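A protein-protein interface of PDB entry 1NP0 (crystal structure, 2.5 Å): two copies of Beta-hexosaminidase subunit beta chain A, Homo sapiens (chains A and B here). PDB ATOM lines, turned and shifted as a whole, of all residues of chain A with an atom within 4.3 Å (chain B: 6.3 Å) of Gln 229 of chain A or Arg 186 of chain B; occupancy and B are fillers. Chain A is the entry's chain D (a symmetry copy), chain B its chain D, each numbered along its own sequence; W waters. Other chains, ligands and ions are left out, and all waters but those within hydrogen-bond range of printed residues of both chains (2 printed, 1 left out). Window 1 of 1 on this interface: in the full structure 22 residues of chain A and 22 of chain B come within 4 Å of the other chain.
The guanidinium group of Arg 218 of chain A lies within salt-bridge range of the side-chain carboxylate of Asp 179 of chain B (2.9 Å). The side-chain amide nitrogen of Asn 182 of chain B sits at hydrogen-bond distance from the side-chain amide oxygen of Gln 229 of chain A, at 3.1 Å. The guanidinium group (NH2) of Arg 186 of chain B lies within hydrogen-bond range of the side-chain amide oxygen (OE1) of Gln 229 of chain A, 3.1 Å away.
The side-chain carboxylate (OD1) of Asp 179 of chain B lies within hydrogen-bond range of the side-chain hydroxyl (OG1) of Thr 181 of chain B, at 2.6 Å. N of Asp 179 of chain B lies within hydrogen-bond range of OD1 of Asn 182 of chain B, 2.9 Å away. The backbone carbonyl oxygen (O) of Pro 185 of chain A lies close to the side-chain amide nitrogen (NE2) of Gln 229 of chain A, 3.4 Å away. O of Trp 188 of chain A sits at hydrogen-bond distance from N of Gln 229 of chain A (3.0 Å). NE of Arg 218 of chain A sits at hydrogen-bond distance from O of Ala 228 of chain A, 2.9 Å away. The guanidinium group (NE) of Arg 218 of chain A lies within hydrogen-bond range of the backbone carbonyl oxygen (O) of Gln 229 of chain A (3.3 Å).
Among the printed residues, pairs that only touch across the chains: Leu 231 of chain A with Tyr 177 of chain B (3.2 Å), Pro 185 of chain A with Thr 181 of chain B (3.3 Å), Gln 229 of chain A with Thr 181 of chain B (3.5 Å), Pro 230 of chain A with Asp 179 of chain B (3.5 Å), Ala 228 of chain A with Thr 181 of chain B (3.6 Å), Arg 218 of chain A with Thr 181 of chain B (3.7 Å), Pro 230 of chain A with Tyr 177 of chain B (3.7 Å), Ala 227 of chain A with Thr 181 of chain B (3.8 Å), Pro 185 of chain A with Asn 182 of chain B (3.9 Å), Pro 230 of chain A with Thr 181 of chain B (3.9 Å) and Pro 230 of chain A with Asn 182 of chain B (3.9 Å).
Gln 229 of chain A touches three residues of chain B. Arg 186 of chain B touches just one residue of chain A: Gln 229 (3.1 Å). Printed residues of chain B within 4 Å of Ala 228 of chain A: Thr 181 (3.6 Å). Of the printed residues of chain B, Pro 185 of chain A touches Thr 181 (3.3 Å) and Asn 182 (3.9 Å). The nearest printed residue of chain A that does not touch Asn 182 of chain B is Ala 227 of chain A (5.9 Å).
Printed residues of chain A that touch a printed residue of chain B: Pro 185, Arg 218, Ala 227, Ala 228, Gln 229, Pro 230 and Leu 231. Printed residues of chain B that touch a printed residue of chain A: Tyr 177, Asp 179, Thr 181, Asn 182 and Arg 186. Hydrophobic or aromatic side chains of chain B within 4 Å of the printed part of chain A: Tyr 177. Among the printed residues, Asp or Glu carboxylates within 4 Å of a Lys or Arg side-chain nitrogen of the other chain: Arg 218 of chain A with Asp 179 of chain B.
6 positions are printed for both chains.
Water W2 lies within hydrogen-bond range of OE1 of Gln 229 of chain A (2.8 Å) and NH2 of Arg 186 of chain B (3.4 Å). Water W1 bridges the guanidinium group of Arg 218 of chain A and the side-chain carboxylate of Asp 179 of chain B.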
ATOM      1  N   PRO A 185      25.477 -18.648   1.522  1.00  0.00           N
ATOM      2  CA  PRO A 185      25.513 -18.900   2.963  1.00  0.00           C
ATOM      3  C   PRO A 185      26.688 -19.772   3.366  1.00  0.00           C
ATOM      4  O   PRO A 185      27.243 -19.527   4.404  1.00  0.00           O
ATOM      5  CB  PRO A 185      24.206 -19.667   3.238  1.00  0.00           C
ATOM      6  CG  PRO A 185      23.383 -19.596   2.009  1.00  0.00           C
ATOM      7  CD  PRO A 185      24.220 -19.135   0.920  1.00  0.00           C
ATOM      8  N   TRP A 188      30.025 -17.257   2.886  1.00  0.00           N
ATOM      9  CA  TRP A 188      30.137 -16.082   3.736  1.00  0.00           C
ATOM     10  C   TRP A 188      29.335 -16.266   5.001  1.00  0.00           C
ATOM     11  O   TRP A 188      28.214 -16.762   4.921  1.00  0.00           O
ATOM     12  CB  TRP A 188      29.620 -14.863   3.001  1.00  0.00           C
ATOM     13  CG  TRP A 188      30.243 -14.700   1.666  1.00  0.00           C
ATOM     14  CD1 TRP A 188      29.648 -14.915   0.470  1.00  0.00           C
ATOM     15  CD2 TRP A 188      31.584 -14.287   1.380  1.00  0.00           C
ATOM     16  NE1 TRP A 188      30.529 -14.654  -0.551  1.00  0.00           N
ATOM     17  CE2 TRP A 188      31.729 -14.273  -0.015  1.00  0.00           C
ATOM     18  CE3 TRP A 188      32.675 -13.907   2.164  1.00  0.00           C
ATOM     19  CZ2 TRP A 188      32.921 -13.917  -0.645  1.00  0.00           C
ATOM     20  CZ3 TRP A 188      33.862 -13.551   1.534  1.00  0.00           C
ATOM     21  CH2 TRP A 188      33.973 -13.562   0.144  1.00  0.00           C
ATOM     22  N   PRO A 189      29.846 -15.871   6.174  1.00  0.00           N
ATOM     23  CA  PRO A 189      31.121 -15.190   6.402  1.00  0.00           C
ATOM     24  C   PRO A 189      32.315 -16.085   6.743  1.00  0.00           C
ATOM     25  O   PRO A 189      33.313 -15.573   7.246  1.00  0.00           O
ATOM     26  CB  PRO A 189      30.772 -14.333   7.613  1.00  0.00           C
ATOM     27  CG  PRO A 189      29.978 -15.271   8.444  1.00  0.00           C
ATOM     28  CD  PRO A 189      29.139 -16.055   7.444  1.00  0.00           C
ATOM     29  N   ARG A 190      32.243 -17.384   6.497  1.00  0.00           N
ATOM     30  CA  ARG A 190      33.398 -18.240   6.783  1.00  0.00           C
ATOM     31  C   ARG A 190      34.646 -17.808   6.019  1.00  0.00           C
ATOM     32  O   ARG A 190      35.731 -17.837   6.578  1.00  0.00           O
ATOM     33  CB  ARG A 190      33.084 -19.705   6.508  1.00  0.00           C
ATOM     34  CG  ARG A 190      32.162 -20.305   7.564  1.00  0.00           C
ATOM     35  CD  ARG A 190      32.046 -21.789   7.524  1.00  0.00           C
ATOM     36  NE  ARG A 190      31.793 -22.173   6.170  1.00  0.00           N
ATOM     37  CZ  ARG A 190      32.270 -23.225   5.531  1.00  0.00           C
ATOM     38  NH1 ARG A 190      33.030 -24.160   6.105  1.00  0.00           N
ATOM     39  NH2 ARG A 190      31.918 -23.347   4.262  1.00  0.00           N
ATOM     40  N   ARG A 218      29.107  -9.199   9.042  1.00  0.00           N
ATOM     41  CA  ARG A 218      28.190 -10.148   8.432  1.00  0.00           C
ATOM     42  C   ARG A 218      26.807  -9.506   8.232  1.00  0.00           C
ATOM     43  O   ARG A 218      26.195  -9.666   7.171  1.00  0.00           O
ATOM     44  CB  ARG A 218      28.124 -11.423   9.274  1.00  0.00           C
ATOM     45  CG  ARG A 218      27.125 -12.438   8.826  1.00  0.00           C
ATOM     46  CD  ARG A 218      25.885 -12.433   9.682  1.00  0.00           C
ATOM     47  NE  ARG A 218      24.753 -13.048   9.010  1.00  0.00           N
ATOM     48  CZ  ARG A 218      23.582 -13.309   9.569  1.00  0.00           C
ATOM     49  NH1 ARG A 218      23.341 -13.005  10.834  1.00  0.00           N
ATOM     50  NH2 ARG A 218      22.638 -13.884   8.837  1.00  0.00           N
ATOM     51  N   ALA A 227      23.593 -13.013   1.289  1.00  0.00           N
ATOM     52  CA  ALA A 227      22.962 -13.819   2.336  1.00  0.00           C
ATOM     53  C   ALA A 227      23.993 -14.607   3.134  1.00  0.00           C
ATOM     54  O   ALA A 227      24.015 -15.836   3.094  1.00  0.00           O
ATOM     55  CB  ALA A 227      21.920 -14.746   1.721  1.00  0.00           C
ATOM     56  N   ALA A 228      24.841 -13.891   3.865  1.00  0.00           N
ATOM     57  CA  ALA A 228      25.861 -14.506   4.697  1.00  0.00           C
ATOM     58  C   ALA A 228      25.198 -15.110   5.935  1.00  0.00           C
ATOM     59  O   ALA A 228      24.349 -14.477   6.573  1.00  0.00           O
ATOM     60  CB  ALA A 228      26.904 -13.481   5.092  1.00  0.00           C
ATOM     61  N   GLN A 229      25.587 -16.335   6.270  1.00  0.00           N
ATOM     62  CA  GLN A 229      24.981 -17.060   7.394  1.00  0.00           C
ATOM     63  C   GLN A 229      25.409 -16.524   8.784  1.00  0.00           C
ATOM     64  O   GLN A 229      26.421 -15.842   8.894  1.00  0.00           O
ATOM     65  CB  GLN A 229      25.261 -18.557   7.240  1.00  0.00           C
ATOM     66  CG  GLN A 229      26.690 -19.011   7.398  1.00  0.00           C
ATOM     67  CD  GLN A 229      26.833 -20.523   7.259  1.00  0.00           C
ATOM     68  OE1 GLN A 229      25.858 -21.247   7.045  1.00  0.00           O
ATOM     69  NE2 GLN A 229      28.046 -20.995   7.384  1.00  0.00           N
ATOM     70  N   PRO A 230      24.664 -16.816   9.848  1.00  0.00           N
ATOM     71  CA  PRO A 230      25.051 -16.317  11.171  1.00  0.00           C
ATOM     72  C   PRO A 230      26.322 -16.939  11.740  1.00  0.00           C
ATOM     73  O   PRO A 230      26.760 -17.999  11.297  1.00  0.00           O
ATOM     74  CB  PRO A 230      23.882 -16.723  12.082  1.00  0.00           C
ATOM     75  CG  PRO A 230      22.927 -17.396  11.294  1.00  0.00           C
ATOM     76  CD  PRO A 230      23.421 -17.593   9.906  1.00  0.00           C
ATOM     77  N   LEU A 231      26.899 -16.252  12.718  1.00  0.00           N
ATOM     78  CA  LEU A 231      28.029 -16.775  13.474  1.00  0.00           C
ATOM     79  C   LEU A 231      27.505 -17.553  14.663  1.00  0.00           C
ATOM     80  O   LEU A 231      28.058 -18.580  15.011  1.00  0.00           O
ATOM     81  CB  LEU A 231      28.981 -15.659  13.943  1.00  0.00           C
ATOM     82  CG  LEU A 231      29.875 -14.963  12.907  1.00  0.00           C
ATOM     83  CD1 LEU A 231      30.897 -14.106  13.587  1.00  0.00           C
ATOM     84  CD2 LEU A 231      30.634 -15.940  12.049  1.00  0.00           C
ATOM     85  N   LEU B 136      19.684 -32.340  12.344  1.00  0.00           N
ATOM     86  CA  LEU B 136      20.066 -31.714  11.078  1.00  0.00           C
ATOM     87  C   LEU B 136      20.861 -30.442  11.271  1.00  0.00           C
ATOM     88  O   LEU B 136      21.508 -29.992  10.346  1.00  0.00           O
ATOM     89  CB  LEU B 136      18.846 -31.469  10.176  1.00  0.00           C
ATOM     90  CG  LEU B 136      17.993 -32.676   9.745  1.00  0.00           C
ATOM     91  CD1 LEU B 136      17.375 -32.437   8.370  1.00  0.00           C
ATOM     92  CD2 LEU B 136      18.747 -33.978   9.719  1.00  0.00           C
ATOM     93  N   ASP B 137      20.806 -29.852  12.451  1.00  0.00           N
ATOM     94  CA  ASP B 137      21.706 -28.763  12.758  1.00  0.00           C
ATOM     95  C   ASP B 137      23.163 -29.254  12.844  1.00  0.00           C
ATOM     96  O   ASP B 137      24.071 -28.488  12.578  1.00  0.00           O
ATOM     97  CB  ASP B 137      21.275 -28.045  14.027  1.00  0.00           C
ATOM     98  CG  ASP B 137      21.291 -28.929  15.233  1.00  0.00           C
ATOM     99  OD1 ASP B 137      20.674 -30.025  15.210  1.00  0.00           O
ATOM    100  OD2 ASP B 137      21.899 -28.591  16.255  1.00  0.00           O
ATOM    101  N   ILE B 139      25.642 -30.408  11.089  1.00  0.00           N
ATOM    102  CA  ILE B 139      26.098 -30.582   9.707  1.00  0.00           C
ATOM    103  C   ILE B 139      27.480 -31.241   9.599  1.00  0.00           C
ATOM    104  O   ILE B 139      28.284 -31.165  10.507  1.00  0.00           O
ATOM    105  CB  ILE B 139      26.073 -29.224   8.946  1.00  0.00           C
ATOM    106  CG1 ILE B 139      26.973 -28.163   9.620  1.00  0.00           C
ATOM    107  CG2 ILE B 139      24.631 -28.742   8.820  1.00  0.00           C
ATOM    108  CD1 ILE B 139      27.331 -27.001   8.737  1.00  0.00           C
ATOM    109  N   LEU B 173      16.136 -29.152  13.525  1.00  0.00           N
ATOM    110  CA  LEU B 173      17.017 -28.106  13.048  1.00  0.00           C
ATOM    111  C   LEU B 173      17.107 -26.985  14.081  1.00  0.00           C
ATOM    112  O   LEU B 173      16.446 -25.961  13.954  1.00  0.00           O
ATOM    113  CB  LEU B 173      16.550 -27.571  11.691  1.00  0.00           C
ATOM    114  CG  LEU B 173      17.510 -26.615  10.977  1.00  0.00           C
ATOM    115  CD1 LEU B 173      18.833 -27.266  10.651  1.00  0.00           C
ATOM    116  CD2 LEU B 173      16.894 -26.156   9.693  1.00  0.00           C
ATOM    117  N   TYR B 177      22.954 -21.712  14.626  1.00  0.00           N
ATOM    118  CA  TYR B 177      23.667 -21.351  13.412  1.00  0.00           C
ATOM    119  C   TYR B 177      22.739 -21.231  12.218  1.00  0.00           C
ATOM    120  O   TYR B 177      23.218 -21.101  11.089  1.00  0.00           O
ATOM    121  CB  TYR B 177      24.763 -22.387  13.160  1.00  0.00           C
ATOM    122  CG  TYR B 177      25.643 -22.530  14.377  1.00  0.00           C
ATOM    123  CD1 TYR B 177      26.525 -21.518  14.730  1.00  0.00           C
ATOM    124  CD2 TYR B 177      25.549 -23.631  15.209  1.00  0.00           C
ATOM    125  CE1 TYR B 177      27.314 -21.621  15.848  1.00  0.00           C
ATOM    126  CE2 TYR B 177      26.326 -23.740  16.337  1.00  0.00           C
ATOM    127  CZ  TYR B 177      27.198 -22.732  16.659  1.00  0.00           C
ATOM    128  OH  TYR B 177      27.975 -22.831  17.791  1.00  0.00           O
ATOM    129  N   VAL B 178      21.426 -21.214  12.473  1.00  0.00           N
ATOM    130  CA  VAL B 178      20.433 -21.167  11.409  1.00  0.00           C
ATOM    131  C   VAL B 178      19.509 -19.948  11.485  1.00  0.00           C
ATOM    132  O   VAL B 178      18.968 -19.642  12.542  1.00  0.00           O
ATOM    133  CB  VAL B 178      19.573 -22.457  11.399  1.00  0.00           C
ATOM    134  CG1 VAL B 178      18.457 -22.372  10.390  1.00  0.00           C
ATOM    135  CG2 VAL B 178      20.438 -23.648  11.064  1.00  0.00           C
ATOM    136  N   ASP B 179      19.339 -19.274  10.352  1.00  0.00           N
ATOM    137  CA  ASP B 179      18.334 -18.232  10.217  1.00  0.00           C
ATOM    138  C   ASP B 179      17.775 -18.269   8.777  1.00  0.00           C
ATOM    139  O   ASP B 179      17.989 -19.254   8.067  1.00  0.00           O
ATOM    140  CB  ASP B 179      18.866 -16.862  10.678  1.00  0.00           C
ATOM    141  CG  ASP B 179      19.821 -16.207   9.713  1.00  0.00           C
ATOM    142  OD1 ASP B 179      20.220 -16.785   8.687  1.00  0.00           O
ATOM    143  OD2 ASP B 179      20.260 -15.067   9.938  1.00  0.00           O
ATOM    144  N   THR B 181      18.728 -16.881   6.054  1.00  0.00           N
ATOM    145  CA  THR B 181      19.744 -16.967   5.006  1.00  0.00           C
ATOM    146  C   THR B 181      20.167 -18.402   4.683  1.00  0.00           C
ATOM    147  O   THR B 181      20.595 -18.668   3.563  1.00  0.00           O
ATOM    148  CB  THR B 181      21.020 -16.189   5.387  1.00  0.00           C
ATOM    149  OG1 THR B 181      21.635 -16.781   6.539  1.00  0.00           O
ATOM    150  CG2 THR B 181      20.737 -14.731   5.788  1.00  0.00           C
ATOM    151  N   ASN B 182      20.035 -19.323   5.638  1.00  0.00           N
ATOM    152  CA  ASN B 182      20.522 -20.685   5.432  1.00  0.00           C
ATOM    153  C   ASN B 182      19.607 -21.870   5.812  1.00  0.00           C
ATOM    154  O   ASN B 182      19.983 -23.011   5.562  1.00  0.00           O
ATOM    155  CB  ASN B 182      21.902 -20.801   6.109  1.00  0.00           C
ATOM    156  CG  ASN B 182      21.832 -20.842   7.623  1.00  0.00           C
ATOM    157  OD1 ASN B 182      20.776 -20.627   8.226  1.00  0.00           O
ATOM    158  ND2 ASN B 182      22.965 -21.135   8.249  1.00  0.00           N
ATOM    159  N   LEU B 183      18.421 -21.604   6.368  1.00  0.00           N
ATOM    160  CA  LEU B 183      17.507 -22.649   6.846  1.00  0.00           C
ATOM    161  C   LEU B 183      17.119 -23.655   5.775  1.00  0.00           C
ATOM    162  O   LEU B 183      17.307 -24.844   5.953  1.00  0.00           O
ATOM    163  CB  LEU B 183      16.231 -22.020   7.422  1.00  0.00           C
ATOM    164  CG  LEU B 183      15.197 -22.966   8.060  1.00  0.00           C
ATOM    165  CD1 LEU B 183      14.609 -22.364   9.291  1.00  0.00           C
ATOM    166  CD2 LEU B 183      14.081 -23.305   7.119  1.00  0.00           C
ATOM    167  N   THR B 184      16.589 -23.161   4.666  1.00  0.00           N
ATOM    168  CA  THR B 184      16.054 -24.021   3.621  1.00  0.00           C
ATOM    169  C   THR B 184      17.062 -24.984   2.992  1.00  0.00           C
ATOM    170  O   THR B 184      16.774 -26.169   2.944  1.00  0.00           O
ATOM    171  CB  THR B 184      15.310 -23.170   2.598  1.00  0.00           C
ATOM    172  OG1 THR B 184      14.182 -22.584   3.251  1.00  0.00           O
ATOM    173  CG2 THR B 184      14.727 -24.010   1.454  1.00  0.00           C
ATOM    174  N   PRO B 185      18.207 -24.503   2.503  1.00  0.00           N
ATOM    175  CA  PRO B 185      19.225 -25.408   1.968  1.00  0.00           C
ATOM    176  C   PRO B 185      19.734 -26.385   3.012  1.00  0.00           C
ATOM    177  O   PRO B 185      19.979 -27.508   2.663  1.00  0.00           O
ATOM    178  CB  PRO B 185      20.377 -24.471   1.559  1.00  0.00           C
ATOM    179  CG  PRO B 185      19.869 -23.082   1.645  1.00  0.00           C
ATOM    180  CD  PRO B 185      18.621 -23.091   2.381  1.00  0.00           C
ATOM    181  N   ARG B 186      19.890 -25.972   4.265  1.00  0.00           N
ATOM    182  CA  ARG B 186      20.325 -26.897   5.309  1.00  0.00           C
ATOM    183  C   ARG B 186      19.277 -27.989   5.584  1.00  0.00           C
ATOM    184  O   ARG B 186      19.628 -29.165   5.735  1.00  0.00           O
ATOM    185  CB  ARG B 186      20.600 -26.136   6.602  1.00  0.00           C
ATOM    186  CG  ARG B 186      21.305 -26.968   7.671  1.00  0.00           C
ATOM    187  CD  ARG B 186      22.120 -26.144   8.666  1.00  0.00           C
ATOM    188  NE  ARG B 186      23.238 -25.442   8.022  1.00  0.00           N
ATOM    189  CZ  ARG B 186      24.103 -24.642   8.634  1.00  0.00           C
ATOM    190  NH1 ARG B 186      24.026 -24.405   9.949  1.00  0.00           N
ATOM    191  NH2 ARG B 186      25.060 -24.061   7.925  1.00  0.00           N
ATOM    192  N   LEU B 187      18.006 -27.591   5.620  1.00  0.00           N
ATOM    193  CA  LEU B 187      16.898 -28.492   5.938  1.00  0.00           C
ATOM    194  C   LEU B 187      16.583 -29.498   4.825  1.00  0.00           C
ATOM    195  O   LEU B 187      16.402 -30.691   5.092  1.00  0.00           O
ATOM    196  CB  LEU B 187      15.602 -27.691   6.248  1.00  0.00           C
ATOM    197  CG  LEU B 187      14.649 -28.096   7.369  1.00  0.00           C
ATOM    198  CD1 LEU B 187      13.294 -27.467   7.199  1.00  0.00           C
ATOM    199  CD2 LEU B 187      14.505 -29.562   7.510  1.00  0.00           C
ATOM    200  N   TRP B 188      16.508 -29.022   3.588  1.00  0.00           N
ATOM    201  CA  TRP B 188      16.091 -29.863   2.476  1.00  0.00           C
ATOM    202  C   TRP B 188      17.226 -30.042   1.496  1.00  0.00           C
ATOM    203  O   TRP B 188      17.907 -29.065   1.200  1.00  0.00           O
ATOM    204  CB  TRP B 188      14.919 -29.227   1.760  1.00  0.00           C
ATOM    205  CG  TRP B 188      13.819 -28.865   2.683  1.00  0.00           C
ATOM    206  CD1 TRP B 188      13.471 -27.616   3.070  1.00  0.00           C
ATOM    207  CD2 TRP B 188      12.914 -29.758   3.345  1.00  0.00           C
ATOM    208  NE1 TRP B 188      12.398 -27.666   3.926  1.00  0.00           N
ATOM    209  CE2 TRP B 188      12.042 -28.974   4.115  1.00  0.00           C
ATOM    210  CE3 TRP B 188      12.738 -31.142   3.348  1.00  0.00           C
ATOM    211  CZ2 TRP B 188      11.026 -29.524   4.897  1.00  0.00           C
ATOM    212  CZ3 TRP B 188      11.724 -31.688   4.126  1.00  0.00           C
ATOM    213  CH2 TRP B 188      10.886 -30.878   4.891  1.00  0.00           C
ATOM    214  N   PRO B 189      17.452 -31.247   0.958  1.00  0.00           N
ATOM    215  CA  PRO B 189      16.668 -32.467   1.151  1.00  0.00           C
ATOM    216  C   PRO B 189      17.152 -33.414   2.253  1.00  0.00           C
ATOM    217  O   PRO B 189      16.745 -34.574   2.257  1.00  0.00           O
ATOM    218  CB  PRO B 189      16.848 -33.139  -0.204  1.00  0.00           C
ATOM    219  CG  PRO B 189      18.288 -32.910  -0.480  1.00  0.00           C
ATOM    220  CD  PRO B 189      18.558 -31.501   0.030  1.00  0.00           C
ATOM    221  N   ARG B 190      18.000 -32.967   3.167  1.00  0.00           N
ATOM    222  CA  ARG B 190      18.435 -33.857   4.247  1.00  0.00           C
ATOM    223  C   ARG B 190      17.267 -34.377   5.080  1.00  0.00           C
ATOM    224  O   ARG B 190      17.267 -35.539   5.453  1.00  0.00           O
ATOM    225  CB  ARG B 190      19.468 -33.180   5.140  1.00  0.00           C
ATOM    226  CG  ARG B 190      20.827 -33.061   4.459  1.00  0.00           C
ATOM    227  CD  ARG B 190      21.949 -32.679   5.363  1.00  0.00           C
ATOM    228  NE  ARG B 190      21.525 -31.554   6.136  1.00  0.00           N
ATOM    229  CZ  ARG B 190      21.783 -31.309   7.407  1.00  0.00           C
ATOM    230  NH1 ARG B 190      22.572 -32.074   8.165  1.00  0.00           N
ATOM    231  NH2 ARG B 190      21.246 -30.211   7.912  1.00  0.00           N
ATOM    232  N   ALA B 191      16.268 -33.526   5.330  1.00  0.00           N
ATOM    233  CA  ALA B 191      15.058 -33.943   6.047  1.00  0.00           C
ATOM    234  C   ALA B 191      14.183 -34.912   5.244  1.00  0.00           C
ATOM    235  O   ALA B 191      13.378 -35.633   5.834  1.00  0.00           O
ATOM    236  CB  ALA B 191      14.251 -32.732   6.468  1.00  0.00           C
ATOM    237  N   ALA B 227      14.472 -23.970  -2.093  1.00  0.00           N
ATOM    238  CA  ALA B 227      15.886 -24.025  -2.466  1.00  0.00           C
ATOM    239  C   ALA B 227      16.610 -25.162  -1.756  1.00  0.00           C
ATOM    240  O   ALA B 227      17.496 -24.930  -0.936  1.00  0.00           O
ATOM    241  CB  ALA B 227      16.553 -22.685  -2.175  1.00  0.00           C
ATOM    242  N   GLN B 229      19.219 -28.049  -1.280  1.00  0.00           N
ATOM    243  CA  GLN B 229      20.610 -28.185  -1.730  1.00  0.00           C
ATOM    244  C   GLN B 229      20.885 -29.492  -2.515  1.00  0.00           C
ATOM    245  O   GLN B 229      20.116 -30.442  -2.415  1.00  0.00           O
ATOM    246  CB  GLN B 229      21.548 -28.024  -0.530  1.00  0.00           C
ATOM    247  CG  GLN B 229      21.520 -29.108   0.518  1.00  0.00           C
ATOM    248  CD  GLN B 229      22.520 -28.852   1.640  1.00  0.00           C
ATOM    249  OE1 GLN B 229      23.249 -27.856   1.640  1.00  0.00           O
ATOM    250  NE2 GLN B 229      22.556 -29.750   2.588  1.00  0.00           N
HETATM  251  O   HOH W   1      20.906 -13.132  12.339  1.00  0.00           O
HETATM  252  O   HOH W   2      25.550 -22.836   4.818  1.00  0.00           O
